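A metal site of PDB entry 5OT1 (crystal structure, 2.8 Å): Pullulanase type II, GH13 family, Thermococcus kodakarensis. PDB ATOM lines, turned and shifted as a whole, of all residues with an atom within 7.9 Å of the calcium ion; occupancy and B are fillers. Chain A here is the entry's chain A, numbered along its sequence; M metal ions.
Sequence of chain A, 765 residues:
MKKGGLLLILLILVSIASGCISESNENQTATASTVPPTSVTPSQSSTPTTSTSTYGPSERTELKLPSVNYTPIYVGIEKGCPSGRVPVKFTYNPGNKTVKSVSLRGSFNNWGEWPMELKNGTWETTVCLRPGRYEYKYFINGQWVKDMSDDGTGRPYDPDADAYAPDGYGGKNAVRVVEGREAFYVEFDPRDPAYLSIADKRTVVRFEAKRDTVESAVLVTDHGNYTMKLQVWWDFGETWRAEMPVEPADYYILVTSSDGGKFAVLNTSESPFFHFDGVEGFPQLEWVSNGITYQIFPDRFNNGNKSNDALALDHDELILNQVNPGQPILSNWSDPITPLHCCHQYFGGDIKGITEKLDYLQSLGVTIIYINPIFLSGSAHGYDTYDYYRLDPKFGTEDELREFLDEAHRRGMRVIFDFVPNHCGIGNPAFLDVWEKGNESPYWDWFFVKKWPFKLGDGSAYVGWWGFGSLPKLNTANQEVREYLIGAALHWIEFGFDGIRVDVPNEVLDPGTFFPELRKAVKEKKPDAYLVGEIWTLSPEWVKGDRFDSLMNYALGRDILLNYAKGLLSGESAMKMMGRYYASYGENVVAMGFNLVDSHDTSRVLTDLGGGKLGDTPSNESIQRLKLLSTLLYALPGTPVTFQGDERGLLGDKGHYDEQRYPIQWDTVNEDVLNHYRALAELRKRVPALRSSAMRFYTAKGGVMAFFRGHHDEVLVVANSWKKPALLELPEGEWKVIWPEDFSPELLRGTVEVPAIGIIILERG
O of Lys 394 sits close to OD1 of Asn 308 (3.4 Å). The side-chain amide oxygen (OD1) of Asn 305 sits at hydrogen-bond distance from the backbone NH (N) of Ser 307. The side-chain amide nitrogen (ND2) of Asn 305 is in hydrogen-bond range of the side-chain carboxylate (OE2) of Glu 400, 3.5 Å away. The side-chain carboxylate of Asp 350 lies within hydrogen-bond range of the backbone NH of Gly 304, 3.0 Å away. The backbone carbonyl oxygen (O) of Asn 302 is in hydrogen-bond range of the backbone NH (N) of Asp 350 (3.2 Å). The backbone NH (N) of Gly 353 is in hydrogen-bond range of the side-chain carboxylate (OD1) of Asp 350 (3.0 Å). OD1 of Asp 299 lies within hydrogen-bond range of N of Gly 348 (3.4 Å).
The nearest printed residue that does not touch the calcium ion is Lys 306 (4.3 Å).
OD1 of Asn 303 binds the calcium ion (2.3 Å). OD1 of Asp 309 is bound to the calcium ion. The side-chain amide oxygen (OD1) of Asn 308 is bound to the calcium ion, 2.3 Å away. O of Asn 305 is bound to the calcium ion, 2.4 Å away. The side-chain carboxylate (OD2) of Asp 350 is bound to the calcium ion (2.5 Å). O of Gly 348 binds the calcium ion, 2.5 Å away.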
ATOM      1  N   PRO A 298      21.892   6.469  18.442  1.00  0.00           N
ATOM      2  CA  PRO A 298      21.231   6.917  17.212  1.00  0.00           C
ATOM      3  C   PRO A 298      20.067   7.878  17.427  1.00  0.00           C
ATOM      4  O   PRO A 298      19.964   8.863  16.689  1.00  0.00           O
ATOM      5  CB  PRO A 298      20.800   5.597  16.560  1.00  0.00           C
ATOM      6  CG  PRO A 298      20.687   4.634  17.671  1.00  0.00           C
ATOM      7  CD  PRO A 298      21.726   5.033  18.685  1.00  0.00           C
ATOM      8  N   ASP A 299      19.201   7.637  18.412  1.00  0.00           N
ATOM      9  CA  ASP A 299      18.046   8.519  18.573  1.00  0.00           C
ATOM     10  C   ASP A 299      18.432   9.925  19.003  1.00  0.00           C
ATOM     11  O   ASP A 299      17.607  10.833  18.925  1.00  0.00           O
ATOM     12  CB  ASP A 299      17.039   7.963  19.583  1.00  0.00           C
ATOM     13  CG  ASP A 299      15.743   8.777  19.623  1.00  0.00           C
ATOM     14  OD1 ASP A 299      14.966   8.695  18.655  1.00  0.00           O
ATOM     15  OD2 ASP A 299      15.518   9.519  20.607  1.00  0.00           O
ATOM     16  N   ASN A 302      21.574  12.437  15.106  1.00  0.00           N
ATOM     17  CA  ASN A 302      21.142  13.288  13.998  1.00  0.00           C
ATOM     18  C   ASN A 302      19.851  12.716  13.423  1.00  0.00           C
ATOM     19  O   ASN A 302      19.766  11.510  13.162  1.00  0.00           O
ATOM     20  CB  ASN A 302      22.239  13.373  12.932  1.00  0.00           C
ATOM     21  CG  ASN A 302      21.857  14.261  11.752  1.00  0.00           C
ATOM     22  OD1 ASN A 302      20.981  15.117  11.863  1.00  0.00           O
ATOM     23  ND2 ASN A 302      22.516  14.059  10.623  1.00  0.00           N
ATOM     24  N   ASN A 303      18.858  13.576  13.240  1.00  0.00           N
ATOM     25  CA  ASN A 303      17.561  13.197  12.658  1.00  0.00           C
ATOM     26  C   ASN A 303      17.599  13.594  11.189  1.00  0.00           C
ATOM     27  O   ASN A 303      17.484  14.777  10.840  1.00  0.00           O
ATOM     28  CB  ASN A 303      16.417  13.875  13.402  1.00  0.00           C
ATOM     29  CG  ASN A 303      15.043  13.480  12.875  1.00  0.00           C
ATOM     30  OD1 ASN A 303      14.779  12.321  12.581  1.00  0.00           O
ATOM     31  ND2 ASN A 303      14.153  14.463  12.756  1.00  0.00           N
ATOM     32  N   GLY A 304      17.792  12.609  10.319  1.00  0.00           N
ATOM     33  CA  GLY A 304      17.847  12.813   8.885  1.00  0.00           C
ATOM     34  C   GLY A 304      16.606  12.381   8.142  1.00  0.00           C
ATOM     35  O   GLY A 304      16.608  12.395   6.905  1.00  0.00           O
ATOM     36  N   ASN A 305      15.551  11.978   8.855  1.00  0.00           N
ATOM     37  CA  ASN A 305      14.319  11.530   8.226  1.00  0.00           C
ATOM     38  C   ASN A 305      13.209  11.734   9.256  1.00  0.00           C
ATOM     39  O   ASN A 305      13.084  10.942  10.198  1.00  0.00           O
ATOM     40  CB  ASN A 305      14.434  10.069   7.803  1.00  0.00           C
ATOM     41  CG  ASN A 305      13.116   9.489   7.302  1.00  0.00           C
ATOM     42  OD1 ASN A 305      12.124  10.205   7.134  1.00  0.00           O
ATOM     43  ND2 ASN A 305      13.096   8.194   7.053  1.00  0.00           N
ATOM     44  N   LYS A 306      12.412  12.789   9.064  1.00  0.00           N
ATOM     45  CA  LYS A 306      11.391  13.094  10.066  1.00  0.00           C
ATOM     46  C   LYS A 306      10.179  12.189   9.981  1.00  0.00           C
ATOM     47  O   LYS A 306       9.364  12.180  10.909  1.00  0.00           O
ATOM     48  CB  LYS A 306      10.979  14.563   9.957  1.00  0.00           C
ATOM     49  CG  LYS A 306      10.482  15.162  11.264  1.00  0.00           C
ATOM     50  CD  LYS A 306      10.748  16.649  11.352  1.00  0.00           C
ATOM     51  CE  LYS A 306      10.441  17.191  12.750  1.00  0.00           C
ATOM     52  NZ  LYS A 306      10.620  18.673  12.832  1.00  0.00           N
ATOM     53  N   SER A 307      10.041  11.411   8.908  1.00  0.00           N
ATOM     54  CA  SER A 307       8.849  10.606   8.662  1.00  0.00           C
ATOM     55  C   SER A 307       8.705   9.444   9.646  1.00  0.00           C
ATOM     56  O   SER A 307       7.578   8.981   9.869  1.00  0.00           O
ATOM     57  CB  SER A 307       8.859  10.074   7.236  1.00  0.00           C
ATOM     58  OG  SER A 307       7.784   9.186   6.997  1.00  0.00           O
ATOM     59  N   ASN A 308       9.801   8.976  10.225  1.00  0.00           N
ATOM     60  CA  ASN A 308       9.770   7.794  11.084  1.00  0.00           C
ATOM     61  C   ASN A 308       9.721   8.134  12.566  1.00  0.00           C
ATOM     62  O   ASN A 308       9.722   7.220  13.399  1.00  0.00           O
ATOM     63  CB  ASN A 308      10.981   6.893  10.785  1.00  0.00           C
ATOM     64  CG  ASN A 308      12.295   7.630  10.819  1.00  0.00           C
ATOM     65  OD1 ASN A 308      12.452   8.621  11.537  1.00  0.00           O
ATOM     66  ND2 ASN A 308      13.271   7.150  10.060  1.00  0.00           N
ATOM     67  N   ASP A 309       9.664   9.425  12.930  1.00  0.00           N
ATOM     68  CA  ASP A 309       9.601   9.800  14.341  1.00  0.00           C
ATOM     69  C   ASP A 309       8.340   9.264  14.998  1.00  0.00           C
ATOM     70  O   ASP A 309       8.372   8.790  16.136  1.00  0.00           O
ATOM     71  CB  ASP A 309       9.672  11.314  14.505  1.00  0.00           C
ATOM     72  CG  ASP A 309      10.915  11.927  13.881  1.00  0.00           C
ATOM     73  OD1 ASP A 309      11.589  11.233  13.105  1.00  0.00           O
ATOM     74  OD2 ASP A 309      11.217  13.098  14.189  1.00  0.00           O
ATOM     75  N   ALA A 310       7.198   9.332  14.301  1.00  0.00           N
ATOM     76  CA  ALA A 310       5.953   8.862  14.877  1.00  0.00           C
ATOM     77  C   ALA A 310       5.903   7.348  15.007  1.00  0.00           C
ATOM     78  O   ALA A 310       5.074   6.833  15.768  1.00  0.00           O
ATOM     79  CB  ALA A 310       4.762   9.342  14.032  1.00  0.00           C
ATOM     80  N   TRP A 333      13.941  18.674  18.537  1.00  0.00           N
ATOM     81  CA  TRP A 333      15.377  18.531  18.758  1.00  0.00           C
ATOM     82  C   TRP A 333      15.866  19.402  19.910  1.00  0.00           C
ATOM     83  O   TRP A 333      16.775  19.020  20.642  1.00  0.00           O
ATOM     84  CB  TRP A 333      16.136  18.851  17.469  1.00  0.00           C
ATOM     85  CG  TRP A 333      17.439  18.135  17.317  1.00  0.00           C
ATOM     86  CD1 TRP A 333      18.683  18.681  17.351  1.00  0.00           C
ATOM     87  CD2 TRP A 333      17.622  16.723  17.112  1.00  0.00           C
ATOM     88  NE1 TRP A 333      19.636  17.707  17.171  1.00  0.00           N
ATOM     89  CE2 TRP A 333      19.006  16.494  17.019  1.00  0.00           C
ATOM     90  CE3 TRP A 333      16.752  15.641  16.989  1.00  0.00           C
ATOM     91  CZ2 TRP A 333      19.548  15.228  16.820  1.00  0.00           C
ATOM     92  CZ3 TRP A 333      17.295  14.375  16.790  1.00  0.00           C
ATOM     93  CH2 TRP A 333      18.674  14.185  16.712  1.00  0.00           C
ATOM     94  N   PHE A 347      13.552  11.930  20.283  1.00  0.00           N
ATOM     95  CA  PHE A 347      13.890  13.162  19.593  1.00  0.00           C
ATOM     96  C   PHE A 347      14.019  13.000  18.079  1.00  0.00           C
ATOM     97  O   PHE A 347      14.133  14.015  17.378  1.00  0.00           O
ATOM     98  CB  PHE A 347      15.203  13.740  20.140  1.00  0.00           C
ATOM     99  CG  PHE A 347      15.112  14.214  21.551  1.00  0.00           C
ATOM    100  CD1 PHE A 347      15.237  13.328  22.608  1.00  0.00           C
ATOM    101  CD2 PHE A 347      14.902  15.551  21.839  1.00  0.00           C
ATOM    102  CE1 PHE A 347      15.149  13.761  23.914  1.00  0.00           C
ATOM    103  CE2 PHE A 347      14.821  15.996  23.136  1.00  0.00           C
ATOM    104  CZ  PHE A 347      14.950  15.095  24.174  1.00  0.00           C
ATOM    105  N   GLY A 348      14.026  11.782  17.570  1.00  0.00           N
ATOM    106  CA  GLY A 348      13.991  11.610  16.132  1.00  0.00           C
ATOM    107  C   GLY A 348      15.125  10.796  15.523  1.00  0.00           C
ATOM    108  O   GLY A 348      14.864   9.975  14.645  1.00  0.00           O
ATOM    109  N   GLY A 349      16.363  11.031  15.983  1.00  0.00           N
ATOM    110  CA  GLY A 349      17.566  10.433  15.427  1.00  0.00           C
ATOM    111  C   GLY A 349      17.385   9.070  14.796  1.00  0.00           C
ATOM    112  O   GLY A 349      16.743   8.193  15.373  1.00  0.00           O
ATOM    113  N   ASP A 350      17.924   8.888  13.592  1.00  0.00           N
ATOM    114  CA  ASP A 350      17.687   7.672  12.820  1.00  0.00           C
ATOM    115  C   ASP A 350      18.968   7.302  12.074  1.00  0.00           C
ATOM    116  O   ASP A 350      20.002   7.960  12.221  1.00  0.00           O
ATOM    117  CB  ASP A 350      16.490   7.857  11.871  1.00  0.00           C
ATOM    118  CG  ASP A 350      16.518   9.192  11.136  1.00  0.00           C
ATOM    119  OD1 ASP A 350      17.600   9.621  10.703  1.00  0.00           O
ATOM    120  OD2 ASP A 350      15.450   9.791  10.974  1.00  0.00           O
ATOM    121  N   ILE A 351      18.889   6.238  11.280  1.00  0.00           N
ATOM    122  CA  ILE A 351      20.050   5.758  10.536  1.00  0.00           C
ATOM    123  C   ILE A 351      20.428   6.725   9.423  1.00  0.00           C
ATOM    124  O   ILE A 351      21.617   6.914   9.134  1.00  0.00           O
ATOM    125  CB  ILE A 351      19.793   4.347   9.992  1.00  0.00           C
ATOM    126  CG1 ILE A 351      19.384   3.407  11.136  1.00  0.00           C
ATOM    127  CG2 ILE A 351      21.010   3.803   9.293  1.00  0.00           C
ATOM    128  CD1 ILE A 351      20.337   3.433  12.302  1.00  0.00           C
ATOM    129  N   LYS A 352      19.446   7.350   8.760  1.00  0.00           N
ATOM    130  CA  LYS A 352      19.762   8.316   7.712  1.00  0.00           C
ATOM    131  C   LYS A 352      20.447   9.551   8.279  1.00  0.00           C
ATOM    132  O   LYS A 352      21.063  10.308   7.522  1.00  0.00           O
ATOM    133  CB  LYS A 352      18.484   8.717   6.959  1.00  0.00           C
ATOM    134  CG  LYS A 352      18.727   9.304   5.566  1.00  0.00           C
ATOM    135  CD  LYS A 352      17.412   9.530   4.817  1.00  0.00           C
ATOM    136  CE  LYS A 352      17.666  10.170   3.451  1.00  0.00           C
ATOM    137  NZ  LYS A 352      16.410  10.524   2.706  1.00  0.00           N
ATOM    138  N   GLY A 353      20.352   9.772   9.589  1.00  0.00           N
ATOM    139  CA  GLY A 353      21.031  10.865  10.241  1.00  0.00           C
ATOM    140  C   GLY A 353      22.522  10.650  10.327  1.00  0.00           C
ATOM    141  O   GLY A 353      23.300  11.597  10.209  1.00  0.00           O
ATOM    142  N   PRO A 393      11.496   0.449  12.974  1.00  0.00           N
ATOM    143  CA  PRO A 393      11.102   1.585  12.123  1.00  0.00           C
ATOM    144  C   PRO A 393      11.404   2.948  12.735  1.00  0.00           C
ATOM    145  O   PRO A 393      11.316   3.948  12.008  1.00  0.00           O
ATOM    146  CB  PRO A 393       9.595   1.377  11.945  1.00  0.00           C
ATOM    147  CG  PRO A 393       9.423  -0.113  12.059  1.00  0.00           C
ATOM    148  CD  PRO A 393      10.399  -0.525  13.126  1.00  0.00           C
ATOM    149  N   LYS A 394      11.753   3.036  14.022  1.00  0.00           N
ATOM    150  CA  LYS A 394      12.164   4.322  14.590  1.00  0.00           C
ATOM    151  C   LYS A 394      13.371   4.885  13.871  1.00  0.00           C
ATOM    152  O   LYS A 394      13.447   6.087  13.608  1.00  0.00           O
ATOM    153  CB  LYS A 394      12.480   4.175  16.072  1.00  0.00           C
ATOM    154  CG  LYS A 394      11.322   3.769  16.942  1.00  0.00           C
ATOM    155  CD  LYS A 394      11.773   3.592  18.388  1.00  0.00           C
ATOM    156  CE  LYS A 394      12.987   2.696  18.482  1.00  0.00           C
ATOM    157  NZ  LYS A 394      13.103   2.167  19.861  1.00  0.00           N
ATOM    158  N   PHE A 395      14.337   4.021  13.536  1.00  0.00           N
ATOM    159  CA  PHE A 395      15.617   4.440  12.975  1.00  0.00           C
ATOM    160  C   PHE A 395      15.708   4.247  11.475  1.00  0.00           C
ATOM    161  O   PHE A 395      16.622   4.811  10.858  1.00  0.00           O
ATOM    162  CB  PHE A 395      16.756   3.673  13.644  1.00  0.00           C
ATOM    163  CG  PHE A 395      16.655   3.604  15.142  1.00  0.00           C
ATOM    164  CD1 PHE A 395      16.866   4.729  15.912  1.00  0.00           C
ATOM    165  CD2 PHE A 395      16.360   2.404  15.773  1.00  0.00           C
ATOM    166  CE1 PHE A 395      16.785   4.675  17.285  1.00  0.00           C
ATOM    167  CE2 PHE A 395      16.278   2.340  17.143  1.00  0.00           C
ATOM    168  CZ  PHE A 395      16.486   3.469  17.904  1.00  0.00           C
ATOM    169  N   GLY A 396      14.831   3.446  10.863  1.00  0.00           N
ATOM    170  CA  GLY A 396      14.826   3.335   9.415  1.00  0.00           C
ATOM    171  C   GLY A 396      14.492   1.971   8.859  1.00  0.00           C
ATOM    172  O   GLY A 396      14.235   1.018   9.599  1.00  0.00           O
ATOM    173  N   GLU A 400      17.649   1.899   4.079  1.00  0.00           N
ATOM    174  CA  GLU A 400      18.412   3.008   4.640  1.00  0.00           C
ATOM    175  C   GLU A 400      19.656   2.504   5.368  1.00  0.00           C
ATOM    176  O   GLU A 400      20.702   3.160   5.343  1.00  0.00           O
ATOM    177  CB  GLU A 400      17.533   3.843   5.571  1.00  0.00           C
ATOM    178  CG  GLU A 400      16.287   4.430   4.919  1.00  0.00           C
ATOM    179  CD  GLU A 400      15.526   5.378   5.839  1.00  0.00           C
ATOM    180  OE1 GLU A 400      16.107   6.410   6.257  1.00  0.00           O
ATOM    181  OE2 GLU A 400      14.347   5.100   6.137  1.00  0.00           O
HETATM  182 CA    CA M   1      13.618  10.348  12.506  1.00  0.00          CA
